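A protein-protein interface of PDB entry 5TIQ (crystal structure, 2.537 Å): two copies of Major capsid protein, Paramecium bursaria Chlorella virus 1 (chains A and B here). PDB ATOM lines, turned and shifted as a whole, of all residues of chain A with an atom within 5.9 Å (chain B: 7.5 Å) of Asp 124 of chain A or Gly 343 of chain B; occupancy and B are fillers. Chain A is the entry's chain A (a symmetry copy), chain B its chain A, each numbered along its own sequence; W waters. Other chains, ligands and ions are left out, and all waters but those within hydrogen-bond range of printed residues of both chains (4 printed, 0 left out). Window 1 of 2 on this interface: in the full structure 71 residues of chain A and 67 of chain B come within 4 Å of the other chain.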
ATOM      1  N   PHE A 119      22.301 -25.246   7.999  1.00  0.00           N
ATOM      2  CA  PHE A 119      21.600 -24.343   7.103  1.00  0.00           C
ATOM      3  C   PHE A 119      21.723 -24.692   5.627  1.00  0.00           C
ATOM      4  O   PHE A 119      20.957 -24.153   4.821  1.00  0.00           O
ATOM      5  CB  PHE A 119      22.077 -22.907   7.344  1.00  0.00           C
ATOM      6  CG  PHE A 119      21.828 -22.432   8.744  1.00  0.00           C
ATOM      7  CD1 PHE A 119      20.547 -22.087   9.151  1.00  0.00           C
ATOM      8  CD2 PHE A 119      22.862 -22.346   9.657  1.00  0.00           C
ATOM      9  CE1 PHE A 119      20.307 -21.658  10.439  1.00  0.00           C
ATOM     10  CE2 PHE A 119      22.630 -21.915  10.949  1.00  0.00           C
ATOM     11  CZ  PHE A 119      21.350 -21.572  11.341  1.00  0.00           C
ATOM     12  N   ARG A 120      22.645 -25.567   5.245  1.00  0.00           N
ATOM     13  CA  ARG A 120      22.628 -26.101   3.893  1.00  0.00           C
ATOM     14  C   ARG A 120      21.870 -27.423   3.876  1.00  0.00           C
ATOM     15  O   ARG A 120      21.731 -28.102   4.897  1.00  0.00           O
ATOM     16  CB  ARG A 120      24.043 -26.295   3.349  1.00  0.00           C
ATOM     17  CG  ARG A 120      24.714 -25.000   2.942  1.00  0.00           C
ATOM     18  CD  ARG A 120      25.797 -25.221   1.905  1.00  0.00           C
ATOM     19  NE  ARG A 120      26.633 -24.034   1.768  1.00  0.00           N
ATOM     20  CZ  ARG A 120      27.665 -23.758   2.558  1.00  0.00           C
ATOM     21  NH1 ARG A 120      27.993 -24.592   3.538  1.00  0.00           N
ATOM     22  NH2 ARG A 120      28.371 -22.650   2.372  1.00  0.00           N
ATOM     23  N   MET A 121      21.362 -27.778   2.699  1.00  0.00           N
ATOM     24  CA  MET A 121      20.532 -28.968   2.586  1.00  0.00           C
ATOM     25  C   MET A 121      20.440 -29.393   1.128  1.00  0.00           C
ATOM     26  O   MET A 121      20.721 -28.613   0.213  1.00  0.00           O
ATOM     27  CB  MET A 121      19.136 -28.720   3.160  1.00  0.00           C
ATOM     28  CG  MET A 121      18.384 -27.601   2.460  1.00  0.00           C
ATOM     29  SD  MET A 121      16.762 -27.314   3.181  1.00  0.00           S
ATOM     30  CE  MET A 121      17.208 -26.387   4.644  1.00  0.00           C
ATOM     31  N   ASN A 122      20.059 -30.652   0.934  1.00  0.00           N
ATOM     32  CA  ASN A 122      19.628 -31.181  -0.365  1.00  0.00           C
ATOM     33  C   ASN A 122      20.788 -31.095  -1.362  1.00  0.00           C
ATOM     34  O   ASN A 122      21.957 -31.245  -0.982  1.00  0.00           O
ATOM     35  CB  ASN A 122      18.364 -30.458  -0.787  1.00  0.00           C
ATOM     36  CG  ASN A 122      17.248 -30.615   0.226  1.00  0.00           C
ATOM     37  OD1 ASN A 122      17.091 -31.679   0.823  1.00  0.00           O
ATOM     38  ND2 ASN A 122      16.476 -29.554   0.437  1.00  0.00           N
ATOM     39  N   ASP A 123      20.474 -30.862  -2.640  1.00  0.00           N
ATOM     40  CA  ASP A 123      21.507 -30.837  -3.671  1.00  0.00           C
ATOM     41  C   ASP A 123      22.503 -29.704  -3.452  1.00  0.00           C
ATOM     42  O   ASP A 123      23.682 -29.845  -3.793  1.00  0.00           O
ATOM     43  CB  ASP A 123      20.866 -30.722  -5.053  1.00  0.00           C
ATOM     44  CG  ASP A 123      20.308 -32.046  -5.552  1.00  0.00           C
ATOM     45  OD1 ASP A 123      20.527 -33.076  -4.880  1.00  0.00           O
ATOM     46  OD2 ASP A 123      19.658 -32.059  -6.619  1.00  0.00           O
ATOM     47  N   ASP A 124      22.049 -28.578  -2.896  1.00  0.00           N
ATOM     48  CA  ASP A 124      22.960 -27.479  -2.585  1.00  0.00           C
ATOM     49  C   ASP A 124      24.057 -27.929  -1.626  1.00  0.00           C
ATOM     50  O   ASP A 124      25.234 -27.601  -1.817  1.00  0.00           O
ATOM     51  CB  ASP A 124      22.164 -26.307  -2.001  1.00  0.00           C
ATOM     52  CG  ASP A 124      23.032 -25.104  -1.670  1.00  0.00           C
ATOM     53  OD1 ASP A 124      23.768 -24.627  -2.563  1.00  0.00           O
ATOM     54  OD2 ASP A 124      22.950 -24.612  -0.522  1.00  0.00           O
ATOM     55  N   ARG A 125      23.691 -28.697  -0.599  1.00  0.00           N
ATOM     56  CA  ARG A 125      24.678 -29.185   0.358  1.00  0.00           C
ATOM     57  C   ARG A 125      25.630 -30.188  -0.283  1.00  0.00           C
ATOM     58  O   ARG A 125      26.823 -30.216   0.044  1.00  0.00           O
ATOM     59  CB  ARG A 125      23.963 -29.808   1.554  1.00  0.00           C
ATOM     60  CG  ARG A 125      24.869 -30.265   2.677  1.00  0.00           C
ATOM     61  CD  ARG A 125      24.089 -31.160   3.621  1.00  0.00           C
ATOM     62  NE  ARG A 125      23.820 -30.514   4.900  1.00  0.00           N
ATOM     63  CZ  ARG A 125      22.838 -30.869   5.721  1.00  0.00           C
ATOM     64  NH1 ARG A 125      22.018 -31.853   5.385  1.00  0.00           N
ATOM     65  NH2 ARG A 125      22.670 -30.231   6.870  1.00  0.00           N
ATOM     66  N   TYR A 126      25.127 -31.020  -1.198  1.00  0.00           N
ATOM     67  CA  TYR A 126      26.005 -31.958  -1.889  1.00  0.00           C
ATOM     68  C   TYR A 126      26.928 -31.232  -2.858  1.00  0.00           C
ATOM     69  O   TYR A 126      28.102 -31.597  -2.999  1.00  0.00           O
ATOM     70  CB  TYR A 126      25.181 -33.017  -2.620  1.00  0.00           C
ATOM     71  CG  TYR A 126      26.014 -33.894  -3.525  1.00  0.00           C
ATOM     72  CD1 TYR A 126      26.978 -34.745  -3.000  1.00  0.00           C
ATOM     73  CD2 TYR A 126      25.841 -33.868  -4.903  1.00  0.00           C
ATOM     74  CE1 TYR A 126      27.747 -35.546  -3.822  1.00  0.00           C
ATOM     75  CE2 TYR A 126      26.604 -34.669  -5.734  1.00  0.00           C
ATOM     76  CZ  TYR A 126      27.555 -35.505  -5.188  1.00  0.00           C
ATOM     77  OH  TYR A 126      28.317 -36.301  -6.011  1.00  0.00           O
ATOM     78  N   ASN A 127      26.414 -30.208  -3.542  1.00  0.00           N
ATOM     79  CA  ASN A 127      27.269 -29.394  -4.397  1.00  0.00           C
ATOM     80  C   ASN A 127      28.357 -28.702  -3.587  1.00  0.00           C
ATOM     81  O   ASN A 127      29.469 -28.498  -4.086  1.00  0.00           O
ATOM     82  CB  ASN A 127      26.426 -28.368  -5.156  1.00  0.00           C
ATOM     83  CG  ASN A 127      27.191 -27.706  -6.286  1.00  0.00           C
ATOM     84  OD1 ASN A 127      27.930 -28.365  -7.020  1.00  0.00           O
ATOM     85  ND2 ASN A 127      27.026 -26.396  -6.425  1.00  0.00           N
ATOM     86  N   TYR A 128      28.061 -28.348  -2.334  1.00  0.00           N
ATOM     87  CA  TYR A 128      29.064 -27.712  -1.489  1.00  0.00           C
ATOM     88  C   TYR A 128      30.200 -28.673  -1.159  1.00  0.00           C
ATOM     89  O   TYR A 128      31.368 -28.269  -1.114  1.00  0.00           O
ATOM     90  CB  TYR A 128      28.417 -27.177  -0.213  1.00  0.00           C
ATOM     91  CG  TYR A 128      29.417 -26.683   0.805  1.00  0.00           C
ATOM     92  CD1 TYR A 128      29.987 -25.419   0.695  1.00  0.00           C
ATOM     93  CD2 TYR A 128      29.793 -27.482   1.877  1.00  0.00           C
ATOM     94  CE1 TYR A 128      30.907 -24.967   1.628  1.00  0.00           C
ATOM     95  CE2 TYR A 128      30.706 -27.041   2.810  1.00  0.00           C
ATOM     96  CZ  TYR A 128      31.261 -25.784   2.684  1.00  0.00           C
ATOM     97  OH  TYR A 128      32.172 -25.350   3.619  1.00  0.00           O
ATOM     98  N   ARG A 129      29.883 -29.949  -0.917  1.00  0.00           N
ATOM     99  CA  ARG A 129      30.947 -30.918  -0.681  1.00  0.00           C
ATOM    100  C   ARG A 129      31.750 -31.183  -1.948  1.00  0.00           C
ATOM    101  O   ARG A 129      32.966 -31.399  -1.871  1.00  0.00           O
ATOM    102  CB  ARG A 129      30.380 -32.228  -0.135  1.00  0.00           C
ATOM    103  CG  ARG A 129      31.474 -33.189   0.315  1.00  0.00           C
ATOM    104  CD  ARG A 129      30.925 -34.404   1.033  1.00  0.00           C
ATOM    105  NE  ARG A 129      32.006 -35.227   1.570  1.00  0.00           N
ATOM    106  CZ  ARG A 129      31.823 -36.356   2.244  1.00  0.00           C
ATOM    107  NH1 ARG A 129      30.596 -36.804   2.466  1.00  0.00           N
ATOM    108  NH2 ARG A 129      32.869 -37.037   2.695  1.00  0.00           N
ATOM    109  N   LEU B 118      20.468 -28.125 -14.840  1.00  0.00           N
ATOM    110  CA  LEU B 118      20.784 -26.835 -14.245  1.00  0.00           C
ATOM    111  C   LEU B 118      19.714 -26.336 -13.283  1.00  0.00           C
ATOM    112  O   LEU B 118      20.039 -25.888 -12.179  1.00  0.00           O
ATOM    113  CB  LEU B 118      21.010 -25.794 -15.348  1.00  0.00           C
ATOM    114  CG  LEU B 118      22.426 -25.742 -15.919  1.00  0.00           C
ATOM    115  CD1 LEU B 118      22.495 -24.780 -17.094  1.00  0.00           C
ATOM    116  CD2 LEU B 118      23.415 -25.347 -14.827  1.00  0.00           C
ATOM    117  N   MET B 121      16.050 -29.844  -9.460  1.00  0.00           N
ATOM    118  CA  MET B 121      16.862 -30.327  -8.354  1.00  0.00           C
ATOM    119  C   MET B 121      16.004 -31.162  -7.414  1.00  0.00           C
ATOM    120  O   MET B 121      14.772 -31.089  -7.435  1.00  0.00           O
ATOM    121  CB  MET B 121      17.505 -29.164  -7.596  1.00  0.00           C
ATOM    122  CG  MET B 121      16.496 -28.196  -7.003  1.00  0.00           C
ATOM    123  SD  MET B 121      17.287 -26.824  -6.150  1.00  0.00           S
ATOM    124  CE  MET B 121      17.769 -25.803  -7.538  1.00  0.00           C
ATOM    125  N   ASN B 122      16.682 -31.970  -6.606  1.00  0.00           N
ATOM    126  CA  ASN B 122      16.091 -32.638  -5.440  1.00  0.00           C
ATOM    127  C   ASN B 122      14.984 -33.590  -5.903  1.00  0.00           C
ATOM    128  O   ASN B 122      15.077 -34.185  -6.985  1.00  0.00           O
ATOM    129  CB  ASN B 122      15.654 -31.580  -4.446  1.00  0.00           C
ATOM    130  CG  ASN B 122      16.806 -30.700  -4.003  1.00  0.00           C
ATOM    131  OD1 ASN B 122      17.927 -31.175  -3.832  1.00  0.00           O
ATOM    132  ND2 ASN B 122      16.540 -29.410  -3.829  1.00  0.00           N
ATOM    133  N   LYS B 335      30.340 -25.681 -11.074  1.00  0.00           N
ATOM    134  CA  LYS B 335      30.065 -25.730  -9.644  1.00  0.00           C
ATOM    135  C   LYS B 335      29.692 -24.372  -9.061  1.00  0.00           C
ATOM    136  O   LYS B 335      28.638 -24.237  -8.434  1.00  0.00           O
ATOM    137  CB  LYS B 335      31.278 -26.288  -8.891  1.00  0.00           C
ATOM    138  CG  LYS B 335      31.608 -27.745  -9.171  1.00  0.00           C
ATOM    139  CD  LYS B 335      32.731 -28.217  -8.251  1.00  0.00           C
ATOM    140  CE  LYS B 335      33.086 -29.679  -8.477  1.00  0.00           C
ATOM    141  NZ  LYS B 335      33.995 -29.872  -9.647  1.00  0.00           N
ATOM    142  N   VAL B 336      30.535 -23.360  -9.267  1.00  0.00           N
ATOM    143  CA  VAL B 336      30.401 -22.098  -8.546  1.00  0.00           C
ATOM    144  C   VAL B 336      29.249 -21.270  -9.097  1.00  0.00           C
ATOM    145  O   VAL B 336      28.426 -20.748  -8.336  1.00  0.00           O
ATOM    146  CB  VAL B 336      31.723 -21.315  -8.598  1.00  0.00           C
ATOM    147  CG1 VAL B 336      31.613 -20.029  -7.791  1.00  0.00           C
ATOM    148  CG2 VAL B 336      32.852 -22.177  -8.096  1.00  0.00           C
ATOM    149  N   GLN B 337      29.192 -21.110 -10.417  1.00  0.00           N
ATOM    150  CA  GLN B 337      28.094 -20.355 -11.013  1.00  0.00           C
ATOM    151  C   GLN B 337      26.723 -20.926 -10.665  1.00  0.00           C
ATOM    152  O   GLN B 337      25.826 -20.132 -10.333  1.00  0.00           O
ATOM    153  CB  GLN B 337      28.294 -20.261 -12.532  1.00  0.00           C
ATOM    154  CG  GLN B 337      29.268 -19.179 -12.961  1.00  0.00           C
ATOM    155  CD  GLN B 337      28.619 -17.808 -13.008  1.00  0.00           C
ATOM    156  OE1 GLN B 337      27.435 -17.682 -13.327  1.00  0.00           O
ATOM    157  NE2 GLN B 337      29.389 -16.774 -12.694  1.00  0.00           N
ATOM    158  N   PRO B 338      26.482 -22.243 -10.706  1.00  0.00           N
ATOM    159  CA  PRO B 338      25.195 -22.738 -10.188  1.00  0.00           C
ATOM    160  C   PRO B 338      25.051 -22.550  -8.688  1.00  0.00           C
ATOM    161  O   PRO B 338      23.947 -22.261  -8.210  1.00  0.00           O
ATOM    162  CB  PRO B 338      25.202 -24.222 -10.585  1.00  0.00           C
ATOM    163  CG  PRO B 338      26.122 -24.288 -11.755  1.00  0.00           C
ATOM    164  CD  PRO B 338      27.209 -23.301 -11.433  1.00  0.00           C
ATOM    165  N   TYR B 339      26.137 -22.704  -7.930  1.00  0.00           N
ATOM    166  CA  TYR B 339      26.057 -22.501  -6.488  1.00  0.00           C
ATOM    167  C   TYR B 339      25.657 -21.071  -6.156  1.00  0.00           C
ATOM    168  O   TYR B 339      24.837 -20.838  -5.261  1.00  0.00           O
ATOM    169  CB  TYR B 339      27.393 -22.846  -5.827  1.00  0.00           C
ATOM    170  CG  TYR B 339      27.435 -22.543  -4.343  1.00  0.00           C
ATOM    171  CD1 TYR B 339      27.012 -23.483  -3.412  1.00  0.00           C
ATOM    172  CD2 TYR B 339      27.900 -21.318  -3.872  1.00  0.00           C
ATOM    173  CE1 TYR B 339      27.046 -23.216  -2.059  1.00  0.00           C
ATOM    174  CE2 TYR B 339      27.932 -21.040  -2.514  1.00  0.00           C
ATOM    175  CZ  TYR B 339      27.503 -21.995  -1.613  1.00  0.00           C
ATOM    176  OH  TYR B 339      27.534 -21.732  -0.259  1.00  0.00           O
ATOM    177  N   GLN B 340      26.230 -20.099  -6.868  1.00  0.00           N
ATOM    178  CA  GLN B 340      26.001 -18.702  -6.528  1.00  0.00           C
ATOM    179  C   GLN B 340      24.621 -18.212  -6.935  1.00  0.00           C
ATOM    180  O   GLN B 340      24.123 -17.250  -6.341  1.00  0.00           O
ATOM    181  CB  GLN B 340      27.066 -17.819  -7.183  1.00  0.00           C
ATOM    182  CG  GLN B 340      28.451 -17.963  -6.582  1.00  0.00           C
ATOM    183  CD  GLN B 340      29.484 -17.103  -7.286  1.00  0.00           C
ATOM    184  OE1 GLN B 340      29.296 -16.700  -8.435  1.00  0.00           O
ATOM    185  NE2 GLN B 340      30.583 -16.813  -6.596  1.00  0.00           N
ATOM    186  N   SER B 341      23.985 -18.843  -7.921  1.00  0.00           N
ATOM    187  CA  SER B 341      22.771 -18.288  -8.498  1.00  0.00           C
ATOM    188  C   SER B 341      21.602 -19.258  -8.618  1.00  0.00           C
ATOM    189  O   SER B 341      20.486 -18.800  -8.886  1.00  0.00           O
ATOM    190  CB  SER B 341      23.071 -17.699  -9.885  1.00  0.00           C
ATOM    191  OG  SER B 341      23.516 -18.702 -10.776  1.00  0.00           O
ATOM    192  N   ILE B 342      21.804 -20.564  -8.423  1.00  0.00           N
ATOM    193  CA  ILE B 342      20.742 -21.556  -8.557  1.00  0.00           C
ATOM    194  C   ILE B 342      20.498 -22.296  -7.247  1.00  0.00           C
ATOM    195  O   ILE B 342      19.354 -22.433  -6.803  1.00  0.00           O
ATOM    196  CB  ILE B 342      21.043 -22.555  -9.697  1.00  0.00           C
ATOM    197  CG1 ILE B 342      21.156 -21.823 -11.035  1.00  0.00           C
ATOM    198  CG2 ILE B 342      19.962 -23.622  -9.765  1.00  0.00           C
ATOM    199  CD1 ILE B 342      21.440 -22.740 -12.198  1.00  0.00           C
ATOM    200  N   GLY B 343      21.561 -22.789  -6.618  1.00  0.00           N
ATOM    201  CA  GLY B 343      21.424 -23.498  -5.361  1.00  0.00           C
ATOM    202  C   GLY B 343      21.036 -24.954  -5.476  1.00  0.00           C
ATOM    203  O   GLY B 343      20.372 -25.484  -4.577  1.00  0.00           O
ATOM    204  N   GLY B 344      21.437 -25.624  -6.552  1.00  0.00           N
ATOM    205  CA  GLY B 344      21.236 -27.054  -6.673  1.00  0.00           C
ATOM    206  C   GLY B 344      22.546 -27.788  -6.867  1.00  0.00           C
ATOM    207  O   GLY B 344      23.536 -27.490  -6.190  1.00  0.00           O
ATOM    208  N   VAL B 345      22.571 -28.749  -7.784  1.00  0.00           N
ATOM    209  CA  VAL B 345      23.815 -29.391  -8.193  1.00  0.00           C
ATOM    210  C   VAL B 345      23.703 -29.739  -9.671  1.00  0.00           C
ATOM    211  O   VAL B 345      22.662 -30.212 -10.138  1.00  0.00           O
ATOM    212  CB  VAL B 345      24.138 -30.631  -7.326  1.00  0.00           C
ATOM    213  CG1 VAL B 345      23.151 -31.760  -7.579  1.00  0.00           C
ATOM    214  CG2 VAL B 345      25.569 -31.099  -7.576  1.00  0.00           C
HETATM  215  O   HOH W   1      24.687 -25.305  -5.104  1.00  0.00           O
HETATM  216  O   HOH W   2      19.180 -27.494  -2.973  1.00  0.00           O
HETATM  217  O   HOH W   3      24.480 -22.477   0.465  1.00  0.00           O
HETATM  218  O   HOH W   4      24.068 -22.250  -2.921  1.00  0.00           O
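Hydrophobic or aromatic side chains of chain B that line the printed part of chain A: Met 121, Tyr 339 and Val 345.
The side-chain sulfur (SD) of Met 121 of chain B sits close to the side-chain amide nitrogen (ND2) of Asn 122 of chain B (3.6 Å). N of Gly 343 of chain B is in hydrogen-bond range of O of Pro 338 of chain B (2.9 Å). The backbone carbonyl oxygen of Arg 120 of chain A is in hydrogen-bond range of the guanidinium group of Arg 125 of chain A (3.1 Å). SD of Met 121 of chain A lies close to ND2 of Asn 122 of chain A (3.6 Å).
Asn 122 of chain A touches its own counterpart, Asn 122 of chain B. Of the 14 pairs that touch across the chains among the printed residues, 1 has its exchanged pair printed and touching as well.
The backbone NH (N) of Asp 123 of chain A lies within hydrogen-bond range of the side-chain amide oxygen (OD1) of Asn 122 of chain B (2.8 Å). O of Lys 335 of chain B is in hydrogen-bond range of ND2 of Asn 127 of chain A. NH2 of Arg 120 of chain A lies within hydrogen-bond range of OH of Tyr 339 of chain B. The backbone carbonyl oxygen (O) of Gly 344 of chain B lies close to the backbone carbonyl oxygen (O) of Asp 123 of chain A (3.4 Å).
Of the printed residues of chain B, Arg 120 of chain A touches Tyr 339 (2.9 Å). Asp 124 of chain A touches three residues of chain B. Of the printed residues of chain A, Asn 122 of chain B touches Asn 122 and Asp 123. Gln 337 of chain B touches none of the printed residues of chain A. Of the printed residues of chain A, Tyr 339 of chain B touches Arg 120, Asp 124 and Asn 127. Ser 341 of chain B touches none of the printed residues of chain A. The nearest residue of chain B that does not touch Asp 124 of chain A is Val 345 of chain B (4.9 Å). The nearest residue of chain A that does not touch Gly 343 of chain B is Asp 123 of chain A (4.9 Å). The nearest printed residue of chain B that does not touch Asn 122 of chain A is Gly 343 of chain B (6.5 Å).
Water W4 bridges the side-chain carboxylate of Asp 124 of chain A and the backbone carbonyl oxygen of Tyr 339 of chain B. Water W1 lies within hydrogen-bond range of O of Gly 344 of chain B (2.7 Å), OD1 of Asp 124 of chain A (2.8 Å) and ND2 of Asn 127 of chain A (2.9 Å). Water W3 lies within hydrogen-bond range of the side-chain carboxylate of Asp 124 of chain A, the guanidinium group of Arg 120 of chain A and the side-chain hydroxyl of Tyr 339 of chain B. Water W2 lies within hydrogen-bond range of the backbone carbonyl oxygen (O) of Gly 343 of chain B (2.8 Å), the backbone NH (N) of Asp 124 of chain A (3.1 Å), the side-chain amide nitrogen (ND2) of Asn 122 of chain B (3.4 Å) and the side-chain sulfur (SD) of Met 121 of chain B (3.8 Å).
CB of Asn 122 of chain A touches OD1 of Asn 122 of chain B, at 3.2 Å. Asp 123 of chain A touches Met 121 of chain B. CG of Asp 123 of chain A touches CG1 of Val 345 of chain B, 3.5 Å away. OD1 of Asp 124 of chain A touches CD1 of Tyr 339 of chain B, 3.5 Å away. Asp 124 of chain A touches Gly 343 of chain B (CB to O, 3.2 Å). Asp 124 of chain A touches Gly 344 of chain B. Val 345 of chain B touches Tyr 126 of chain A (CG2 to CD2, 3.9 Å). ND2 of Asn 127 of chain A touches CB of Tyr 339 of chain B, at 3.6 Å. Asn 127 of chain A touches Gly 344 of chain B (CB to O, 3.2 Å). CG2 of Val 345 of chain B touches OD1 of Asn 127 of chain A, at 3.7 Å.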
